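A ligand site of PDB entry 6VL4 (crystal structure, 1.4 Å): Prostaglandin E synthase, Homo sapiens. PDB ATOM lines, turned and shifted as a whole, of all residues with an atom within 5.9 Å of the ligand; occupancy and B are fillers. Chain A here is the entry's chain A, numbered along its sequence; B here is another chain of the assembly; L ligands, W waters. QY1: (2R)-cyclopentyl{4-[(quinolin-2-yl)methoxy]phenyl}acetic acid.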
ATOM      1  N   ASN A  76      16.672 -23.122 -14.698  1.00  0.00           N
ATOM      2  CA  ASN A  76      16.444 -23.892 -13.482  1.00  0.00           C
ATOM      3  C   ASN A  76      15.214 -24.785 -13.637  1.00  0.00           C
ATOM      4  O   ASN A  76      15.211 -25.918 -13.167  1.00  0.00           O
ATOM      5  CB  ASN A  76      16.417 -23.003 -12.231  1.00  0.00           C
ATOM      6  CG  ASN A  76      16.378 -23.807 -10.957  1.00  0.00           C
ATOM      7  OD1 ASN A  76      15.301 -24.120 -10.450  1.00  0.00           O
ATOM      8  ND2 ASN A  76      17.541 -24.135 -10.412  1.00  0.00           N
ATOM      9  N   HIS A 115       8.990 -21.018  -6.761  1.00  0.00           N
ATOM     10  CA  HIS A 115      10.342 -20.753  -7.240  1.00  0.00           C
ATOM     11  C   HIS A 115      10.336 -19.645  -8.288  1.00  0.00           C
ATOM     12  O   HIS A 115      11.158 -18.739  -8.223  1.00  0.00           O
ATOM     13  CB  HIS A 115      11.019 -22.036  -7.760  1.00  0.00           C
ATOM     14  CG  HIS A 115      12.453 -21.837  -8.120  1.00  0.00           C
ATOM     15  ND1 HIS A 115      12.847 -21.395  -9.368  1.00  0.00           N
ATOM     16  CD2 HIS A 115      13.584 -22.007  -7.402  1.00  0.00           C
ATOM     17  CE1 HIS A 115      14.158 -21.300  -9.401  1.00  0.00           C
ATOM     18  NE2 HIS A 115      14.638 -21.667  -8.199  1.00  0.00           N
ATOM     19  N   ARG A 128      14.024 -18.261  -2.596  1.00  0.00           N
ATOM     20  CA  ARG A 128      14.116 -18.985  -3.856  1.00  0.00           C
ATOM     21  C   ARG A 128      14.846 -20.319  -3.646  1.00  0.00           C
ATOM     22  O   ARG A 128      14.362 -21.357  -4.106  1.00  0.00           O
ATOM     23  CB  ARG A 128      14.801 -18.141  -4.930  1.00  0.00           C
ATOM     24  CG  ARG A 128      14.790 -18.757  -6.315  1.00  0.00           C
ATOM     25  CD  ARG A 128      15.832 -18.140  -7.221  1.00  0.00           C
ATOM     26  NE  ARG A 128      17.189 -18.546  -6.920  1.00  0.00           N
ATOM     27  CZ  ARG A 128      18.120 -17.790  -6.336  1.00  0.00           C
ATOM     28  NH1 ARG A 128      17.868 -16.538  -5.987  1.00  0.00           N
ATOM     29  NH2 ARG A 128      19.327 -18.292  -6.119  1.00  0.00           N
ATOM     30  N   SER A 129      15.994 -20.274  -2.960  1.00  0.00           N
ATOM     31  CA  SER A 129      16.843 -21.446  -2.768  1.00  0.00           C
ATOM     32  C   SER A 129      16.127 -22.511  -1.949  1.00  0.00           C
ATOM     33  O   SER A 129      16.316 -23.706  -2.194  1.00  0.00           O
ATOM     34  CB  SER A 129      18.178 -21.063  -2.180  1.00  0.00           C
ATOM     35  OG  SER A 129      18.912 -20.261  -3.089  1.00  0.00           O
ATOM     36  N   TYR A 132      13.506 -24.227  -4.191  1.00  0.00           N
ATOM     37  CA  TYR A 132      14.260 -25.090  -5.082  1.00  0.00           C
ATOM     38  C   TYR A 132      14.554 -26.421  -4.381  1.00  0.00           C
ATOM     39  O   TYR A 132      14.217 -27.482  -4.916  1.00  0.00           O
ATOM     40  CB  TYR A 132      15.491 -24.329  -5.576  1.00  0.00           C
ATOM     41  CG  TYR A 132      16.590 -25.072  -6.298  1.00  0.00           C
ATOM     42  CD1 TYR A 132      16.347 -26.118  -7.186  1.00  0.00           C
ATOM     43  CD2 TYR A 132      17.906 -24.661  -6.142  1.00  0.00           C
ATOM     44  CE1 TYR A 132      17.389 -26.757  -7.836  1.00  0.00           C
ATOM     45  CE2 TYR A 132      18.960 -25.284  -6.791  1.00  0.00           C
ATOM     46  CZ  TYR A 132      18.692 -26.336  -7.653  1.00  0.00           C
ATOM     47  OH  TYR A 132      19.733 -26.961  -8.296  1.00  0.00           O
ATOM     48  N   THR A 133      15.132 -26.334  -3.179  1.00  0.00           N
ATOM     49  CA  THR A 133      15.552 -27.485  -2.402  1.00  0.00           C
ATOM     50  C   THR A 133      14.326 -28.335  -2.032  1.00  0.00           C
ATOM     51  O   THR A 133      14.369 -29.559  -2.178  1.00  0.00           O
ATOM     52  CB  THR A 133      16.391 -27.057  -1.190  1.00  0.00           C
ATOM     53  OG1 THR A 133      17.463 -26.225  -1.641  1.00  0.00           O
ATOM     54  CG2 THR A 133      16.980 -28.224  -0.421  1.00  0.00           C
ATOM     55  N   GLN A 136      12.877 -30.365  -4.792  1.00  0.00           N
ATOM     56  CA  GLN A 136      13.764 -31.446  -5.199  1.00  0.00           C
ATOM     57  C   GLN A 136      13.520 -32.697  -4.350  1.00  0.00           C
ATOM     58  O   GLN A 136      13.819 -33.805  -4.809  1.00  0.00           O
ATOM     59  CB  GLN A 136      15.234 -31.036  -5.160  1.00  0.00           C
ATOM     60  CG  GLN A 136      15.648 -30.059  -6.259  1.00  0.00           C
ATOM     61  CD  GLN A 136      15.342 -30.523  -7.658  1.00  0.00           C
ATOM     62  OE1 GLN A 136      14.217 -30.403  -8.150  1.00  0.00           O
ATOM     63  NE2 GLN A 136      16.356 -31.039  -8.332  1.00  0.00           N
ATOM     64  N   LEU A 137      12.978 -32.521  -3.140  1.00  0.00           N
ATOM     65  CA  LEU A 137      12.839 -33.616  -2.188  1.00  0.00           C
ATOM     66  C   LEU A 137      11.900 -34.707  -2.705  1.00  0.00           C
ATOM     67  O   LEU A 137      12.295 -35.880  -2.671  1.00  0.00           O
ATOM     68  CB  LEU A 137      12.439 -33.089  -0.803  1.00  0.00           C
ATOM     69  CG  LEU A 137      13.483 -32.248  -0.067  1.00  0.00           C
ATOM     70  CD1 LEU A 137      12.898 -31.638   1.193  1.00  0.00           C
ATOM     71  CD2 LEU A 137      14.728 -33.073   0.272  1.00  0.00           C
ATOM     72  N   ALA A 140      13.773 -36.661  -5.401  1.00  0.00           N
ATOM     73  CA  ALA A 140      14.762 -37.561  -4.830  1.00  0.00           C
ATOM     74  C   ALA A 140      14.076 -38.841  -4.337  1.00  0.00           C
ATOM     75  O   ALA A 140      14.571 -39.942  -4.581  1.00  0.00           O
ATOM     76  CB  ALA A 140      15.505 -36.868  -3.707  1.00  0.00           C
ATOM     77  N   TYR B  30      21.698 -34.409 -10.342  1.00  0.00           N
ATOM     78  CA  TYR B  30      21.430 -33.791  -9.053  1.00  0.00           C
ATOM     79  C   TYR B  30      22.730 -33.524  -8.299  1.00  0.00           C
ATOM     80  O   TYR B  30      22.858 -32.497  -7.630  1.00  0.00           O
ATOM     81  CB  TYR B  30      20.470 -34.632  -8.218  1.00  0.00           C
ATOM     82  CG  TYR B  30      19.042 -34.707  -8.713  1.00  0.00           C
ATOM     83  CD1 TYR B  30      18.520 -33.740  -9.569  1.00  0.00           C
ATOM     84  CD2 TYR B  30      18.206 -35.731  -8.295  1.00  0.00           C
ATOM     85  CE1 TYR B  30      17.203 -33.814 -10.016  1.00  0.00           C
ATOM     86  CE2 TYR B  30      16.885 -35.803  -8.713  1.00  0.00           C
ATOM     87  CZ  TYR B  30      16.388 -34.841  -9.588  1.00  0.00           C
ATOM     88  OH  TYR B  30      15.086 -34.902 -10.012  1.00  0.00           O
ATOM     89  N   ALA B  33      24.181 -30.436  -9.655  1.00  0.00           N
ATOM     90  CA  ALA B  33      23.415 -29.298  -9.166  1.00  0.00           C
ATOM     91  C   ALA B  33      23.882 -28.893  -7.766  1.00  0.00           C
ATOM     92  O   ALA B  33      24.009 -27.702  -7.484  1.00  0.00           O
ATOM     93  CB  ALA B  33      21.941 -29.605  -9.190  1.00  0.00           C
ATOM     94  N   ILE B  34      24.130 -29.890  -6.911  1.00  0.00           N
ATOM     95  CA  ILE B  34      24.559 -29.657  -5.535  1.00  0.00           C
ATOM     96  C   ILE B  34      25.979 -29.107  -5.524  1.00  0.00           C
ATOM     97  O   ILE B  34      26.258 -28.133  -4.820  1.00  0.00           O
ATOM     98  CB  ILE B  34      24.366 -30.922  -4.673  1.00  0.00           C
ATOM     99  CG1 ILE B  34      22.886 -31.281  -4.516  1.00  0.00           C
ATOM    100  CG2 ILE B  34      25.037 -30.773  -3.306  1.00  0.00           C
ATOM    101  CD1 ILE B  34      22.614 -32.733  -4.180  1.00  0.00           C
ATOM    102  N   THR B  36      27.423 -27.418  -7.842  1.00  0.00           N
ATOM    103  CA  THR B  36      27.325 -26.044  -8.323  1.00  0.00           C
ATOM    104  C   THR B  36      27.114 -25.075  -7.162  1.00  0.00           C
ATOM    105  O   THR B  36      27.807 -24.072  -7.061  1.00  0.00           O
ATOM    106  CB  THR B  36      26.248 -25.879  -9.405  1.00  0.00           C
ATOM    107  OG1 THR B  36      26.511 -26.777 -10.486  1.00  0.00           O
ATOM    108  CG2 THR B  36      26.164 -24.475  -9.943  1.00  0.00           C
ATOM    109  N   GLY B  37      26.135 -25.398  -6.301  1.00  0.00           N
ATOM    110  CA  GLY B  37      25.816 -24.599  -5.121  1.00  0.00           C
ATOM    111  C   GLY B  37      27.000 -24.477  -4.165  1.00  0.00           C
ATOM    112  O   GLY B  37      27.289 -23.391  -3.666  1.00  0.00           O
ATOM    113  N   GLN B  38      27.676 -25.605  -3.924  1.00  0.00           N
ATOM    114  CA  GLN B  38      28.831 -25.686  -3.038  1.00  0.00           C
ATOM    115  C   GLN B  38      29.953 -24.778  -3.545  1.00  0.00           C
ATOM    116  O   GLN B  38      30.583 -24.088  -2.749  1.00  0.00           O
ATOM    117  CB  GLN B  38      29.312 -27.130  -2.872  1.00  0.00           C
ATOM    118  CG  GLN B  38      28.345 -28.014  -2.092  1.00  0.00           C
ATOM    119  CD  GLN B  38      28.738 -29.474  -2.071  1.00  0.00           C
ATOM    120  OE1 GLN B  38      29.342 -29.995  -3.020  1.00  0.00           O
ATOM    121  NE2 GLN B  38      28.385 -30.156  -1.003  1.00  0.00           N
ATOM    122  N   ARG B  40      29.631 -22.162  -5.598  1.00  0.00           N
ATOM    123  CA  ARG B  40      29.174 -20.783  -5.494  1.00  0.00           C
ATOM    124  C   ARG B  40      29.466 -20.232  -4.094  1.00  0.00           C
ATOM    125  O   ARG B  40      29.946 -19.104  -3.968  1.00  0.00           O
ATOM    126  CB  ARG B  40      27.672 -20.657  -5.795  1.00  0.00           C
ATOM    127  CG  ARG B  40      27.326 -20.724  -7.278  1.00  0.00           C
ATOM    128  CD  ARG B  40      25.939 -20.146  -7.527  1.00  0.00           C
ATOM    129  NE  ARG B  40      25.581 -20.168  -8.943  1.00  0.00           N
ATOM    130  CZ  ARG B  40      25.935 -19.252  -9.846  1.00  0.00           C
ATOM    131  NH1 ARG B  40      26.742 -18.254  -9.524  1.00  0.00           N
ATOM    132  NH2 ARG B  40      25.477 -19.342 -11.084  1.00  0.00           N
ATOM    133  N   LEU B  41      29.189 -21.034  -3.068  1.00  0.00           N
ATOM    134  CA  LEU B  41      29.344 -20.629  -1.683  1.00  0.00           C
ATOM    135  C   LEU B  41      30.827 -20.541  -1.304  1.00  0.00           C
ATOM    136  O   LEU B  41      31.227 -19.610  -0.605  1.00  0.00           O
ATOM    137  CB  LEU B  41      28.586 -21.614  -0.773  1.00  0.00           C
ATOM    138  CG  LEU B  41      27.070 -21.463  -0.750  1.00  0.00           C
ATOM    139  CD1 LEU B  41      26.400 -22.753  -0.297  1.00  0.00           C
ATOM    140  CD2 LEU B  41      26.637 -20.302   0.133  1.00  0.00           C
ATOM    141  N   PHE B  46      28.020 -15.407  -6.994  1.00  0.00           N
ATOM    142  CA  PHE B  46      26.569 -15.527  -7.104  1.00  0.00           C
ATOM    143  C   PHE B  46      26.089 -14.807  -8.348  1.00  0.00           C
ATOM    144  O   PHE B  46      26.718 -13.863  -8.807  1.00  0.00           O
ATOM    145  CB  PHE B  46      25.911 -15.040  -5.810  1.00  0.00           C
ATOM    146  CG  PHE B  46      26.475 -15.686  -4.568  1.00  0.00           C
ATOM    147  CD1 PHE B  46      26.076 -16.955  -4.178  1.00  0.00           C
ATOM    148  CD2 PHE B  46      27.447 -15.030  -3.816  1.00  0.00           C
ATOM    149  CE1 PHE B  46      26.620 -17.558  -3.055  1.00  0.00           C
ATOM    150  CE2 PHE B  46      27.985 -15.641  -2.693  1.00  0.00           C
ATOM    151  CZ  PHE B  46      27.570 -16.896  -2.313  1.00  0.00           C
ATOM    152  N   ASN B  48      22.873 -13.673  -8.604  1.00  0.00           N
ATOM    153  CA  ASN B  48      21.765 -12.812  -8.210  1.00  0.00           C
ATOM    154  C   ASN B  48      22.203 -11.872  -7.086  1.00  0.00           C
ATOM    155  O   ASN B  48      22.805 -12.326  -6.114  1.00  0.00           O
ATOM    156  CB  ASN B  48      20.548 -13.633  -7.754  1.00  0.00           C
ATOM    157  CG  ASN B  48      20.044 -14.575  -8.814  1.00  0.00           C
ATOM    158  OD1 ASN B  48      19.561 -14.147  -9.870  1.00  0.00           O
ATOM    159  ND2 ASN B  48      20.147 -15.871  -8.550  1.00  0.00           N
ATOM    160  N   ASP B  51      21.282 -12.952  -3.581  1.00  0.00           N
ATOM    161  CA  ASP B  51      22.138 -14.014  -3.073  1.00  0.00           C
ATOM    162  C   ASP B  51      23.431 -13.409  -2.502  1.00  0.00           C
ATOM    163  O   ASP B  51      23.830 -13.761  -1.395  1.00  0.00           O
ATOM    164  CB  ASP B  51      22.462 -15.073  -4.130  1.00  0.00           C
ATOM    165  CG  ASP B  51      21.270 -15.778  -4.748  1.00  0.00           C
ATOM    166  OD1 ASP B  51      20.169 -15.710  -4.165  1.00  0.00           O
ATOM    167  OD2 ASP B  51      21.450 -16.386  -5.826  1.00  0.00           O
ATOM    168  N   HIS B  55      25.318 -13.235   1.362  1.00  0.00           N
ATOM    169  CA  HIS B  55      26.531 -14.030   1.533  1.00  0.00           C
ATOM    170  C   HIS B  55      27.797 -13.169   1.422  1.00  0.00           C
ATOM    171  O   HIS B  55      28.814 -13.655   0.925  1.00  0.00           O
ATOM    172  CB  HIS B  55      26.535 -15.199   0.537  1.00  0.00           C
ATOM    173  CG  HIS B  55      25.490 -16.221   0.803  1.00  0.00           C
ATOM    174  ND1 HIS B  55      25.568 -17.107   1.853  1.00  0.00           N
ATOM    175  CD2 HIS B  55      24.341 -16.518   0.146  1.00  0.00           C
ATOM    176  CE1 HIS B  55      24.510 -17.897   1.848  1.00  0.00           C
ATOM    177  NE2 HIS B  55      23.749 -17.559   0.800  1.00  0.00           N
HETATM  178  C7  QY1 L   1      17.845 -32.260  -2.901  1.00  0.00           C
HETATM  179  C6  QY1 L   1      22.225 -24.298  -5.409  1.00  0.00           C
HETATM  180  C1  QY1 L   1      17.903 -34.068  -4.496  1.00  0.00           C
HETATM  181  C5  QY1 L   1      20.548 -23.975  -3.695  1.00  0.00           C
HETATM  182  C4  QY1 L   1      19.469 -31.027  -5.957  1.00  0.00           C
HETATM  183  C3  QY1 L   1      18.540 -33.230  -5.404  1.00  0.00           C
HETATM  184  C2  QY1 L   1      17.558 -33.579  -3.237  1.00  0.00           C
HETATM  185  C8  QY1 L   1      20.370 -25.353  -3.595  1.00  0.00           C
HETATM  186  C9  QY1 L   1      22.047 -25.677  -5.308  1.00  0.00           C
HETATM  187  C10 QY1 L   1      19.740 -29.722  -5.579  1.00  0.00           C
HETATM  188  C11 QY1 L   1      18.827 -31.898  -5.062  1.00  0.00           C
HETATM  189  C12 QY1 L   1      21.468 -23.454  -4.589  1.00  0.00           C
HETATM  190  C13 QY1 L   1      18.486 -31.401  -3.789  1.00  0.00           C
HETATM  191  C14 QY1 L   1      21.126 -26.196  -4.401  1.00  0.00           C
HETATM  192  C15 QY1 L   1      19.367 -29.325  -4.312  1.00  0.00           C
HETATM  193  C16 QY1 L   1      20.804 -21.519  -5.923  1.00  0.00           C
HETATM  194  C17 QY1 L   1      22.959 -19.380  -3.394  1.00  0.00           C
HETATM  195  C18 QY1 L   1      23.441 -20.520  -2.497  1.00  0.00           C
HETATM  196  C19 QY1 L   1      23.092 -19.878  -4.833  1.00  0.00           C
HETATM  197  C20 QY1 L   1      23.804 -21.676  -3.423  1.00  0.00           C
HETATM  198  C21 QY1 L   1      23.034 -21.399  -4.711  1.00  0.00           C
HETATM  199  C22 QY1 L   1      19.633 -27.930  -3.861  1.00  0.00           C
HETATM  200  C23 QY1 L   1      21.610 -21.948  -4.693  1.00  0.00           C
HETATM  201  N24 QY1 L   1      18.739 -30.132  -3.418  1.00  0.00           N
HETATM  202  O25 QY1 L   1      21.214 -21.445  -7.070  1.00  0.00           O
HETATM  203  O26 QY1 L   1      19.513 -21.247  -5.595  1.00  0.00           O
HETATM  204  O27 QY1 L   1      20.936 -27.541  -4.289  1.00  0.00           O
HETATM  205  O   HOH W   1      17.509 -21.327  -7.581  1.00  0.00           O
HETATM  206  O   HOH W   2      19.694 -21.751  -9.231  1.00  0.00           O
HETATM  207  O   HOH W   3      22.158 -19.348  -8.620  1.00  0.00           O
HETATM  208  O   HOH W   4      22.209 -25.762  -8.550  1.00  0.00           O
HETATM  209  O   HOH W   5      23.525 -22.728  -8.471  1.00  0.00           O
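OG of Ser 129 lies within hydrogen-bond range of O26 of the ligand, 2.8 Å away.
The guanidinium group (NH2) of Arg 128 is in salt-bridge range of an oxygen (O26) of the ligand (3.0 Å).
O of Ser 129 is in hydrogen-bond range of OG1 of Thr 133 (2.8 Å).
The guanidinium group (NH2) of Arg 128 is in salt-bridge range of the side-chain carboxylate (OD2) of Asp 51 of chain B (2.9 Å).
The guanidinium group of Arg 128 lies close to the side-chain amide nitrogen of Asn 48 of chain B (3.5 Å).
The side-chain amide nitrogen (ND2) of Asn 48 of chain B lies within hydrogen-bond range of the side-chain carboxylate (OD2) of Asp 51 of chain B, at 3.1 Å.
Tyr 132 touches the ligand (CE2 to C14, 3.4 Å).
Thr 133 touches the ligand (OG1 to C22, 3.5 Å).
Gln 136 touches the ligand (CB to C13, 3.5 Å).
Ala 140 touches the ligand.
CG of Tyr 30 of chain B touches C3 of the ligand, at 3.7 Å.
Ala 33 of chain B touches the ligand (O to C9, 3.6 Å).
Ile 34 of chain B touches the ligand (CG1 to C10, 3.7 Å).
Gly 37 of chain B touches the ligand (CA to C6, 3.6 Å).
CD of Arg 40 of chain B touches C19 of the ligand, at 3.9 Å.
Asp 51 of chain B touches the ligand (OD2 to C19, 3.98 Å).
Hydrophobic or aromatic side chains within 4 Å of the ligand: Tyr 132, Ala 140, Tyr 30 of chain B and Ile 34 of chain B.
Water W2 bridges O25 of the ligand (2.7 Å) and ND2 of Asn 76 (3.4 Å).
Water W1 lies within hydrogen-bond range of an oxygen (O26) of the ligand (2.8 Å), the guanidinium group (NE) of Arg 128 (2.9 Å) and a ring nitrogen (NE2) of His 115 (3.0 Å).
Water W5 lies within hydrogen-bond range of an oxygen (O25) of the ligand (3.0 Å) and the guanidinium group of Arg 40 of chain B (3.3 Å).
Water W4 lies within hydrogen-bond range of the side-chain hydroxyl (OH) of Tyr 132 (2.8 Å) and the backbone carbonyl oxygen (O) of Ala 33 of chain B (2.9 Å).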
